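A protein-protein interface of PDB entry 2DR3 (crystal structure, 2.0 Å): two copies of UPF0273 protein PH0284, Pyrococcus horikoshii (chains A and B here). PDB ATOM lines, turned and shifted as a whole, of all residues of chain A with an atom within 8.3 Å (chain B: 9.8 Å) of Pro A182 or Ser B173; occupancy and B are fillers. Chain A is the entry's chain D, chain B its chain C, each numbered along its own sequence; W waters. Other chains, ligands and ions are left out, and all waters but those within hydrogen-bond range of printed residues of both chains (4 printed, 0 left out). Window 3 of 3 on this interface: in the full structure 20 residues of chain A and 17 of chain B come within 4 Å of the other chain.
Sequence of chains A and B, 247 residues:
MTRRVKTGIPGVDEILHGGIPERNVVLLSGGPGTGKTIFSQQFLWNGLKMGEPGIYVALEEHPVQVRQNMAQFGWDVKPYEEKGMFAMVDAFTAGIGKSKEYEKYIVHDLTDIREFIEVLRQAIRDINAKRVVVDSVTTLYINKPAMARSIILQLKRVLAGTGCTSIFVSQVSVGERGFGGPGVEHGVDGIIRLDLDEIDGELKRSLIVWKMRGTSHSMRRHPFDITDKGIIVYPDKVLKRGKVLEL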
ATOM      1  N   TYR A 141      13.793   6.639  -1.669  1.00  0.00           N
ATOM      2  CA  TYR A 141      12.386   6.194  -1.756  1.00  0.00           C
ATOM      3  C   TYR A 141      11.847   6.042  -3.196  1.00  0.00           C
ATOM      4  O   TYR A 141      10.678   5.761  -3.444  1.00  0.00           O
ATOM      5  CB  TYR A 141      11.485   7.148  -0.958  1.00  0.00           C
ATOM      6  CG  TYR A 141      11.792   8.562  -1.271  1.00  0.00           C
ATOM      7  CD1 TYR A 141      11.422   9.093  -2.500  1.00  0.00           C
ATOM      8  CD2 TYR A 141      12.394   9.379  -0.312  1.00  0.00           C
ATOM      9  CE1 TYR A 141      11.643  10.432  -2.769  1.00  0.00           C
ATOM     10  CE2 TYR A 141      12.622  10.713  -0.594  1.00  0.00           C
ATOM     11  CZ  TYR A 141      12.258  11.237  -1.815  1.00  0.00           C
ATOM     12  OH  TYR A 141      12.542  12.555  -2.113  1.00  0.00           O
ATOM     13  N   PRO A 145       7.626   5.101  -3.193  1.00  0.00           N
ATOM     14  CA  PRO A 145       7.080   6.462  -3.102  1.00  0.00           C
ATOM     15  C   PRO A 145       6.187   6.799  -1.908  1.00  0.00           C
ATOM     16  O   PRO A 145       6.111   7.956  -1.500  1.00  0.00           O
ATOM     17  CB  PRO A 145       6.365   6.639  -4.443  1.00  0.00           C
ATOM     18  CG  PRO A 145       6.032   5.233  -4.853  1.00  0.00           C
ATOM     19  CD  PRO A 145       7.284   4.497  -4.493  1.00  0.00           C
ATOM     20  N   ALA A 146       5.513   5.800  -1.347  1.00  0.00           N
ATOM     21  CA  ALA A 146       4.642   6.035  -0.199  1.00  0.00           C
ATOM     22  C   ALA A 146       5.444   6.323   1.076  1.00  0.00           C
ATOM     23  O   ALA A 146       4.920   6.877   2.036  1.00  0.00           O
ATOM     24  CB  ALA A 146       3.732   4.828   0.014  1.00  0.00           C
ATOM     25  N   MET A 147       6.716   5.946   1.073  1.00  0.00           N
ATOM     26  CA  MET A 147       7.602   6.145   2.220  1.00  0.00           C
ATOM     27  C   MET A 147       8.309   7.493   2.189  1.00  0.00           C
ATOM     28  O   MET A 147       8.900   7.910   3.182  1.00  0.00           O
ATOM     29  CB  MET A 147       8.675   5.050   2.248  1.00  0.00           C
ATOM     30  CG  MET A 147       8.133   3.635   2.365  1.00  0.00           C
ATOM     31  SD  MET A 147       7.218   3.440   3.892  1.00  0.00           S
ATOM     32  CE  MET A 147       8.541   3.815   5.086  1.00  0.00           C
ATOM     33  N   ALA A 148       8.262   8.170   1.045  1.00  0.00           N
ATOM     34  CA  ALA A 148       8.940   9.453   0.906  1.00  0.00           C
ATOM     35  C   ALA A 148       8.610  10.438   2.024  1.00  0.00           C
ATOM     36  O   ALA A 148       9.513  11.006   2.652  1.00  0.00           O
ATOM     37  CB  ALA A 148       8.612  10.073  -0.449  1.00  0.00           C
ATOM     38  N   ARG A 149       7.320  10.641   2.279  1.00  0.00           N
ATOM     39  CA  ARG A 149       6.897  11.594   3.307  1.00  0.00           C
ATOM     40  C   ARG A 149       7.554  11.400   4.677  1.00  0.00           C
ATOM     41  O   ARG A 149       8.180  12.320   5.207  1.00  0.00           O
ATOM     42  CB  ARG A 149       5.375  11.564   3.484  1.00  0.00           C
ATOM     43  CG  ARG A 149       4.893  12.561   4.543  1.00  0.00           C
ATOM     44  CD  ARG A 149       3.382  12.684   4.589  1.00  0.00           C
ATOM     45  NE  ARG A 149       2.962  13.809   5.430  1.00  0.00           N
ATOM     46  CZ  ARG A 149       2.993  13.809   6.759  1.00  0.00           C
ATOM     47  NH1 ARG A 149       3.420  12.742   7.421  1.00  0.00           N
ATOM     48  NH2 ARG A 149       2.594  14.882   7.427  1.00  0.00           N
ATOM     49  N   SER A 150       7.406  10.210   5.256  1.00  0.00           N
ATOM     50  CA  SER A 150       7.989   9.956   6.571  1.00  0.00           C
ATOM     51  C   SER A 150       9.512  10.033   6.539  1.00  0.00           C
ATOM     52  O   SER A 150      10.129  10.571   7.460  1.00  0.00           O
ATOM     53  CB  SER A 150       7.544   8.593   7.112  1.00  0.00           C
ATOM     54  OG  SER A 150       8.038   7.532   6.323  1.00  0.00           O
ATOM     55  N   ILE A 152      11.400  11.826   4.571  1.00  0.00           N
ATOM     56  CA  ILE A 152      11.755  13.234   4.496  1.00  0.00           C
ATOM     57  C   ILE A 152      11.614  13.927   5.848  1.00  0.00           C
ATOM     58  O   ILE A 152      12.511  14.655   6.284  1.00  0.00           O
ATOM     59  CB  ILE A 152      10.855  13.983   3.475  1.00  0.00           C
ATOM     60  CG1 ILE A 152      11.253  13.614   2.045  1.00  0.00           C
ATOM     61  CG2 ILE A 152      10.957  15.470   3.690  1.00  0.00           C
ATOM     62  CD1 ILE A 152      12.608  14.105   1.646  1.00  0.00           C
ATOM     63  N   GLU A 176      10.104  16.939 -16.414  1.00  0.00           N
ATOM     64  CA  GLU A 176       9.189  16.885 -15.287  1.00  0.00           C
ATOM     65  C   GLU A 176       9.109  18.237 -14.588  1.00  0.00           C
ATOM     66  O   GLU A 176      10.104  18.919 -14.383  1.00  0.00           O
ATOM     67  CB  GLU A 176       9.696  15.823 -14.310  1.00  0.00           C
ATOM     68  CG  GLU A 176       8.958  15.862 -12.971  1.00  0.00           C
ATOM     69  CD  GLU A 176       7.476  15.678 -13.211  1.00  0.00           C
ATOM     70  OE1 GLU A 176       7.114  14.825 -14.008  1.00  0.00           O
ATOM     71  OE2 GLU A 176       6.692  16.396 -12.593  1.00  0.00           O
ATOM     72  N   ARG A 177       7.845  18.622 -14.293  1.00  0.00           N
ATOM     73  CA  ARG A 177       7.628  19.989 -13.875  1.00  0.00           C
ATOM     74  C   ARG A 177       7.855  20.219 -12.383  1.00  0.00           C
ATOM     75  O   ARG A 177       8.208  21.297 -11.947  1.00  0.00           O
ATOM     76  CB  ARG A 177       6.190  20.448 -14.217  1.00  0.00           C
ATOM     77  CG  ARG A 177       5.127  19.386 -13.993  1.00  0.00           C
ATOM     78  CD  ARG A 177       3.753  19.894 -14.454  1.00  0.00           C
ATOM     79  NE  ARG A 177       3.402  21.146 -13.773  1.00  0.00           N
ATOM     80  CZ  ARG A 177       2.251  21.745 -14.139  1.00  0.00           C
ATOM     81  NH1 ARG A 177       1.490  21.204 -15.076  1.00  0.00           N
ATOM     82  NH2 ARG A 177       1.876  22.879 -13.542  1.00  0.00           N
ATOM     83  N   GLY A 178       7.596  19.153 -11.602  1.00  0.00           N
ATOM     84  CA  GLY A 178       7.358  19.334 -10.196  1.00  0.00           C
ATOM     85  C   GLY A 178       8.662  19.035  -9.511  1.00  0.00           C
ATOM     86  O   GLY A 178       9.699  19.482  -9.984  1.00  0.00           O
ATOM     87  N   PHE A 179       8.784  18.667  -8.240  1.00  0.00           N
ATOM     88  CA  PHE A 179      10.029  18.826  -7.499  1.00  0.00           C
ATOM     89  C   PHE A 179      10.448  17.498  -6.888  1.00  0.00           C
ATOM     90  O   PHE A 179      11.595  17.336  -6.465  1.00  0.00           O
ATOM     91  CB  PHE A 179       9.847  19.847  -6.378  1.00  0.00           C
ATOM     92  CG  PHE A 179       9.242  21.145  -6.830  1.00  0.00           C
ATOM     93  CD1 PHE A 179       9.931  21.980  -7.702  1.00  0.00           C
ATOM     94  CD2 PHE A 179       7.989  21.538  -6.368  1.00  0.00           C
ATOM     95  CE1 PHE A 179       9.385  23.194  -8.108  1.00  0.00           C
ATOM     96  CE2 PHE A 179       7.428  22.752  -6.768  1.00  0.00           C
ATOM     97  CZ  PHE A 179       8.128  23.583  -7.638  1.00  0.00           C
ATOM     98  N   GLY A 180       9.506  16.560  -6.842  1.00  0.00           N
ATOM     99  CA  GLY A 180       9.768  15.248  -6.276  1.00  0.00           C
ATOM    100  C   GLY A 180       8.476  14.542  -5.905  1.00  0.00           C
ATOM    101  O   GLY A 180       8.485  13.418  -5.404  1.00  0.00           O
ATOM    102  N   GLY A 181       7.357  15.222  -6.142  1.00  0.00           N
ATOM    103  CA  GLY A 181       6.063  14.636  -5.844  1.00  0.00           C
ATOM    104  C   GLY A 181       5.530  14.826  -4.430  1.00  0.00           C
ATOM    105  O   GLY A 181       6.209  15.434  -3.589  1.00  0.00           O
ATOM    106  N   PRO A 182       4.277  14.318  -4.196  1.00  0.00           N
ATOM    107  CA  PRO A 182       3.466  14.260  -2.958  1.00  0.00           C
ATOM    108  C   PRO A 182       4.314  13.634  -1.896  1.00  0.00           C
ATOM    109  O   PRO A 182       4.627  12.424  -1.903  1.00  0.00           O
ATOM    110  CB  PRO A 182       2.301  13.345  -3.339  1.00  0.00           C
ATOM    111  CG  PRO A 182       2.206  13.499  -4.774  1.00  0.00           C
ATOM    112  CD  PRO A 182       3.566  13.762  -5.318  1.00  0.00           C
ATOM    113  N   GLY A 183       4.681  14.477  -0.951  1.00  0.00           N
ATOM    114  CA  GLY A 183       5.509  14.077   0.152  1.00  0.00           C
ATOM    115  C   GLY A 183       6.608  15.103   0.124  1.00  0.00           C
ATOM    116  O   GLY A 183       6.462  16.194   0.676  1.00  0.00           O
ATOM    117  N   VAL A 184       7.678  14.759  -0.540  1.00  0.00           N
ATOM    118  CA  VAL A 184       8.852  15.606  -0.664  1.00  0.00           C
ATOM    119  C   VAL A 184       8.640  17.148  -0.641  1.00  0.00           C
ATOM    120  O   VAL A 184       9.075  17.804   0.300  1.00  0.00           O
ATOM    121  CB  VAL A 184       9.579  15.151  -1.919  1.00  0.00           C
ATOM    122  CG1 VAL A 184      10.916  15.831  -2.050  1.00  0.00           C
ATOM    123  CG2 VAL A 184       9.707  13.641  -1.848  1.00  0.00           C
ATOM    124  N   GLU A 185       7.929  17.693  -1.614  1.00  0.00           N
ATOM    125  CA  GLU A 185       7.762  19.136  -1.696  1.00  0.00           C
ATOM    126  C   GLU A 185       7.030  19.878  -0.575  1.00  0.00           C
ATOM    127  O   GLU A 185       7.313  21.045  -0.365  1.00  0.00           O
ATOM    128  CB  GLU A 185       7.172  19.504  -3.068  1.00  0.00           C
ATOM    129  CG  GLU A 185       5.877  18.822  -3.470  1.00  0.00           C
ATOM    130  CD  GLU A 185       5.577  19.053  -4.953  1.00  0.00           C
ATOM    131  OE1 GLU A 185       6.319  18.513  -5.811  1.00  0.00           O
ATOM    132  OE2 GLU A 185       4.613  19.780  -5.256  1.00  0.00           O
ATOM    133  N   HIS A 186       6.118  19.234   0.143  1.00  0.00           N
ATOM    134  CA  HIS A 186       5.424  19.916   1.255  1.00  0.00           C
ATOM    135  C   HIS A 186       6.211  19.771   2.571  1.00  0.00           C
ATOM    136  O   HIS A 186       6.101  20.605   3.468  1.00  0.00           O
ATOM    137  CB  HIS A 186       4.017  19.344   1.459  1.00  0.00           C
ATOM    138  CG  HIS A 186       3.165  19.393   0.230  1.00  0.00           C
ATOM    139  ND1 HIS A 186       2.672  20.573  -0.285  1.00  0.00           N
ATOM    140  CD2 HIS A 186       2.759  18.413  -0.614  1.00  0.00           C
ATOM    141  CE1 HIS A 186       2.001  20.318  -1.396  1.00  0.00           C
ATOM    142  NE2 HIS A 186       2.040  19.016  -1.618  1.00  0.00           N
ATOM    143  N   GLY A 187       7.008  18.708   2.670  1.00  0.00           N
ATOM    144  CA  GLY A 187       7.778  18.458   3.881  1.00  0.00           C
ATOM    145  C   GLY A 187       9.079  19.228   4.076  1.00  0.00           C
ATOM    146  O   GLY A 187       9.572  19.341   5.197  1.00  0.00           O
ATOM    147  N   SER B  29      -6.775  25.391  -0.385  1.00  0.00           N
ATOM    148  CA  SER B  29      -6.010  24.553  -1.294  1.00  0.00           C
ATOM    149  C   SER B  29      -4.923  25.251  -2.110  1.00  0.00           C
ATOM    150  O   SER B  29      -5.117  26.356  -2.615  1.00  0.00           O
ATOM    151  CB  SER B  29      -7.004  23.860  -2.240  1.00  0.00           C
ATOM    152  OG  SER B  29      -6.350  23.133  -3.255  1.00  0.00           O
ATOM    153  N   GLY B  30      -3.784  24.579  -2.254  1.00  0.00           N
ATOM    154  CA  GLY B  30      -2.687  25.131  -3.030  1.00  0.00           C
ATOM    155  C   GLY B  30      -1.427  24.280  -2.986  1.00  0.00           C
ATOM    156  O   GLY B  30      -1.310  23.354  -2.164  1.00  0.00           O
ATOM    157  N   GLY B  31      -0.489  24.587  -3.878  1.00  0.00           N
ATOM    158  CA  GLY B  31       0.763  23.849  -3.931  1.00  0.00           C
ATOM    159  C   GLY B  31       1.697  24.289  -2.823  1.00  0.00           C
ATOM    160  O   GLY B  31       1.356  25.178  -2.042  1.00  0.00           O
ATOM    161  N   PRO B  32       2.894  23.697  -2.723  1.00  0.00           N
ATOM    162  CA  PRO B  32       3.827  24.071  -1.660  1.00  0.00           C
ATOM    163  C   PRO B  32       4.298  25.523  -1.795  1.00  0.00           C
ATOM    164  O   PRO B  32       4.447  26.103  -2.878  1.00  0.00           O
ATOM    165  CB  PRO B  32       5.025  23.139  -1.750  1.00  0.00           C
ATOM    166  CG  PRO B  32       5.090  22.658  -3.176  1.00  0.00           C
ATOM    167  CD  PRO B  32       3.543  22.676  -3.540  1.00  0.00           C
ATOM    168  N   GLY B  33       4.523  26.132  -0.597  1.00  0.00           N
ATOM    169  CA  GLY B  33       4.924  27.537  -0.525  1.00  0.00           C
ATOM    170  C   GLY B  33       3.907  28.518  -1.143  1.00  0.00           C
ATOM    171  O   GLY B  33       4.267  29.536  -1.722  1.00  0.00           O
ATOM    172  N   THR B  34       2.602  28.195  -1.039  1.00  0.00           N
ATOM    173  CA  THR B  34       1.623  29.168  -1.527  1.00  0.00           C
ATOM    174  C   THR B  34       1.141  30.118  -0.415  1.00  0.00           C
ATOM    175  O   THR B  34       0.475  31.114  -0.656  1.00  0.00           O
ATOM    176  CB  THR B  34       0.435  28.449  -2.174  1.00  0.00           C
ATOM    177  OG1 THR B  34       0.175  27.226  -1.485  1.00  0.00           O
ATOM    178  CG2 THR B  34       0.749  28.139  -3.640  1.00  0.00           C
ATOM    179  N   LYS B  36      -0.388  28.785   2.528  1.00  0.00           N
ATOM    180  CA  LYS B  36      -1.515  28.164   3.230  1.00  0.00           C
ATOM    181  C   LYS B  36      -1.314  28.085   4.758  1.00  0.00           C
ATOM    182  O   LYS B  36      -2.241  28.255   5.539  1.00  0.00           O
ATOM    183  CB  LYS B  36      -1.724  26.766   2.640  1.00  0.00           C
ATOM    184  CG  LYS B  36      -1.971  26.816   1.131  1.00  0.00           C
ATOM    185  CD  LYS B  36      -2.097  25.426   0.508  1.00  0.00           C
ATOM    186  CE  LYS B  36      -1.029  24.449   1.027  1.00  0.00           C
ATOM    187  NZ  LYS B  36       0.256  24.717   0.370  1.00  0.00           N
ATOM    188  N   GLU B  60       1.769  18.324  10.038  1.00  0.00           N
ATOM    189  CA  GLU B  60       2.970  18.494   9.212  1.00  0.00           C
ATOM    190  C   GLU B  60       4.241  18.834   9.986  1.00  0.00           C
ATOM    191  O   GLU B  60       5.345  18.517   9.538  1.00  0.00           O
ATOM    192  CB  GLU B  60       2.737  19.581   8.153  1.00  0.00           C
ATOM    193  CG  GLU B  60       1.427  19.443   7.372  1.00  0.00           C
ATOM    194  CD  GLU B  60       1.210  18.056   6.788  1.00  0.00           C
ATOM    195  OE1 GLU B  60       2.090  17.560   6.040  1.00  0.00           O
ATOM    196  OE2 GLU B  60       0.146  17.468   7.077  1.00  0.00           O
ATOM    197  N   THR B 138      -5.141  16.624   4.212  1.00  0.00           N
ATOM    198  CA  THR B 138      -4.659  15.722   3.160  1.00  0.00           C
ATOM    199  C   THR B 138      -3.861  14.550   3.753  1.00  0.00           C
ATOM    200  O   THR B 138      -3.858  13.430   3.230  1.00  0.00           O
ATOM    201  CB  THR B 138      -3.698  16.454   2.185  1.00  0.00           C
ATOM    202  OG1 THR B 138      -4.335  17.616   1.642  1.00  0.00           O
ATOM    203  CG2 THR B 138      -3.296  15.527   1.049  1.00  0.00           C
ATOM    204  N   THR B 139      -3.167  14.829   4.842  1.00  0.00           N
ATOM    205  CA  THR B 139      -2.351  13.824   5.490  1.00  0.00           C
ATOM    206  C   THR B 139      -3.161  12.681   6.090  1.00  0.00           C
ATOM    207  O   THR B 139      -2.682  11.544   6.129  1.00  0.00           O
ATOM    208  CB  THR B 139      -1.456  14.480   6.541  1.00  0.00           C
ATOM    209  OG1 THR B 139      -0.559  15.371   5.868  1.00  0.00           O
ATOM    210  CG2 THR B 139      -0.638  13.438   7.313  1.00  0.00           C
ATOM    211  N   ILE B 142      -3.891  10.624   2.677  1.00  0.00           N
ATOM    212  CA  ILE B 142      -2.956  10.606   1.562  1.00  0.00           C
ATOM    213  C   ILE B 142      -2.698   9.211   0.977  1.00  0.00           C
ATOM    214  O   ILE B 142      -2.428   9.081  -0.220  1.00  0.00           O
ATOM    215  CB  ILE B 142      -1.613  11.276   1.958  1.00  0.00           C
ATOM    216  CG1 ILE B 142      -0.766  11.514   0.709  1.00  0.00           C
ATOM    217  CG2 ILE B 142      -0.869  10.414   2.968  1.00  0.00           C
ATOM    218  CD1 ILE B 142      -1.471  12.329  -0.374  1.00  0.00           C
ATOM    219  N   ASN B 143      -2.797   8.171   1.803  1.00  0.00           N
ATOM    220  CA  ASN B 143      -2.582   6.809   1.318  1.00  0.00           C
ATOM    221  C   ASN B 143      -3.890   6.029   1.168  1.00  0.00           C
ATOM    222  O   ASN B 143      -3.895   4.888   0.690  1.00  0.00           O
ATOM    223  CB  ASN B 143      -1.627   6.041   2.243  1.00  0.00           C
ATOM    224  CG  ASN B 143      -0.225   6.628   2.252  1.00  0.00           C
ATOM    225  OD1 ASN B 143       0.357   6.898   1.198  1.00  0.00           O
ATOM    226  ND2 ASN B 143       0.329   6.819   3.444  1.00  0.00           N
ATOM    227  N   SER B 170      -5.261  21.948   2.384  1.00  0.00           N
ATOM    228  CA  SER B 170      -5.170  20.868   1.402  1.00  0.00           C
ATOM    229  C   SER B 170      -3.913  21.068   0.553  1.00  0.00           C
ATOM    230  O   SER B 170      -3.802  22.046  -0.192  1.00  0.00           O
ATOM    231  CB  SER B 170      -6.420  20.893   0.500  1.00  0.00           C
ATOM    232  OG  SER B 170      -6.414  19.842  -0.449  1.00  0.00           O
ATOM    233  N   GLN B 171      -2.970  20.143   0.666  1.00  0.00           N
ATOM    234  CA  GLN B 171      -1.734  20.230  -0.092  1.00  0.00           C
ATOM    235  C   GLN B 171      -1.937  19.578  -1.454  1.00  0.00           C
ATOM    236  O   GLN B 171      -2.317  18.409  -1.544  1.00  0.00           O
ATOM    237  CB  GLN B 171      -0.598  19.521   0.663  1.00  0.00           C
ATOM    238  CG  GLN B 171      -0.535  19.889   2.145  1.00  0.00           C
ATOM    239  CD  GLN B 171       0.624  19.253   2.887  1.00  0.00           C
ATOM    240  OE1 GLN B 171       0.895  18.063   2.744  1.00  0.00           O
ATOM    241  NE2 GLN B 171       1.310  20.048   3.696  1.00  0.00           N
ATOM    242  N   VAL B 172      -1.707  20.344  -2.516  1.00  0.00           N
ATOM    243  CA  VAL B 172      -1.779  19.832  -3.878  1.00  0.00           C
ATOM    244  C   VAL B 172      -0.403  19.864  -4.539  1.00  0.00           C
ATOM    245  O   VAL B 172       0.424  20.727  -4.278  1.00  0.00           O
ATOM    246  CB  VAL B 172      -2.767  20.692  -4.670  1.00  0.00           C
ATOM    247  CG1 VAL B 172      -4.091  20.808  -3.914  1.00  0.00           C
ATOM    248  CG2 VAL B 172      -2.193  22.079  -4.887  1.00  0.00           C
ATOM    249  N   SER B 173      -0.154  18.852  -5.384  1.00  0.00           N
ATOM    250  CA  SER B 173       1.179  18.702  -5.959  1.00  0.00           C
ATOM    251  C   SER B 173       1.174  18.895  -7.480  1.00  0.00           C
ATOM    252  O   SER B 173       2.183  19.216  -8.104  1.00  0.00           O
ATOM    253  CB  SER B 173       1.677  17.300  -5.614  1.00  0.00           C
ATOM    254  OG  SER B 173       1.237  16.953  -4.299  1.00  0.00           O
ATOM    255  N   ARG B 193      -8.451  28.990  -3.072  1.00  0.00           N
ATOM    256  CA  ARG B 193      -7.235  28.485  -3.698  1.00  0.00           C
ATOM    257  C   ARG B 193      -6.161  29.555  -3.650  1.00  0.00           C
ATOM    258  O   ARG B 193      -6.413  30.732  -3.969  1.00  0.00           O
ATOM    259  CB  ARG B 193      -7.522  28.086  -5.151  1.00  0.00           C
ATOM    260  CG  ARG B 193      -6.290  27.769  -6.012  1.00  0.00           C
ATOM    261  CD  ARG B 193      -5.411  26.697  -5.380  1.00  0.00           C
ATOM    262  NE  ARG B 193      -4.221  26.339  -6.153  1.00  0.00           N
ATOM    263  CZ  ARG B 193      -4.196  25.493  -7.185  1.00  0.00           C
ATOM    264  NH1 ARG B 193      -5.304  24.897  -7.609  1.00  0.00           N
ATOM    265  NH2 ARG B 193      -3.041  25.207  -7.780  1.00  0.00           N
HETATM  266  O   HOH W   1       2.047  22.880   1.323  1.00  0.00           O
HETATM  267  O   HOH W   2       4.446  18.182   5.007  1.00  0.00           O
HETATM  268  O   HOH W   3       4.468  16.841  -8.047  1.00  0.00           O
HETATM  269  O   HOH W   4       3.857  21.683   4.358  1.00  0.00           O
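The guanidinium group (NH2) of Arg A149 lies within salt-bridge range of the side-chain carboxylate (OE1) of Glu B60 (3.1 Å). OG of Ser B173 sits at hydrogen-bond distance from NE2 of His A186, 3.5 Å away.
N of Val B172 sits at hydrogen-bond distance from O of Gly B30 (3.1 Å). OE2 of Glu B60 lies within hydrogen-bond range of OG1 of Thr B139, 2.5 Å away. The backbone NH (N) of Gln B171 sits at hydrogen-bond distance from the side-chain hydroxyl (OG1) of Thr B138, 3.0 Å away. The backbone NH (N) of Phe A179 lies within hydrogen-bond range of the side-chain carboxylate (OE1) of Glu A185, 3.5 Å away. The side-chain carboxylate (OE1) of Glu A185 sits at hydrogen-bond distance from the backbone NH (N) of Gly A181.
Thr B139 touches Arg A149 (CG2 to NH2, 3.5 Å). Pro A182 touches Ser B173 (CG to OG, 3.6 Å). Pro B32 touches Glu A185. Glu A185 touches Ser B173 (OE2 to CA, 3.7 Å). Pro B32 touches His A186 (CD to CE1, 3.5 Å). Gln B171 touches His A186 (CB to CE1, 3.4 Å). CE1 of His A186 touches O of Val B172 (3.3 Å).
Pro A182 touches just one residue of chain B: Ser B173 (3.6 Å). Ser B173 touches just these residues of chain A: Pro A182 (3.6 Å), Glu A185 (3.7 Å) and His A186 (3.5 Å). No residue of chain B comes within 4 Å of Gly A181. No residue of chain B comes within 4 Å of Gly A183. Of the printed residues of chain A, Glu B60 touches Arg A149. Printed residues of chain B within 4 Å of Arg A149: Glu B60 (3.1 Å) and Thr B139 (3.5 Å). Printed residues of chain B within 4 Å of Glu A185: Pro B32 (3.4 Å) and Ser B173 (3.7 Å). Of the printed residues of chain A, Pro B32 touches Glu A185 (3.4 Å) and His A186 (3.5 Å). Of the printed residues of chain A, Gln B171 touches His A186. Ile A152 touches none of the printed residues of chain B. Ser A150 touches none of the printed residues of chain B. The nearest printed residue of chain A that does not touch Glu B60 is His A186 (5.3 Å).
Of the 17 printed residues of chain B, 6 touch a printed residue of chain A.
No position is printed for both chains.
Water W4 lies within hydrogen-bond range of the backbone carbonyl oxygen of His A186 (2.6 Å) and the side-chain amide nitrogen of Gln B171 (3.1 Å). Water W2 bridges OE1 of Glu B60 and O of His A186. Water W1 lies within hydrogen-bond range of NZ of Lys B36 (2.7 Å) and ND1 of His A186 (2.9 Å). Water W3 bridges O of Ser B173 (3.3 Å) and OE1 of Glu A185 (3.3 Å).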
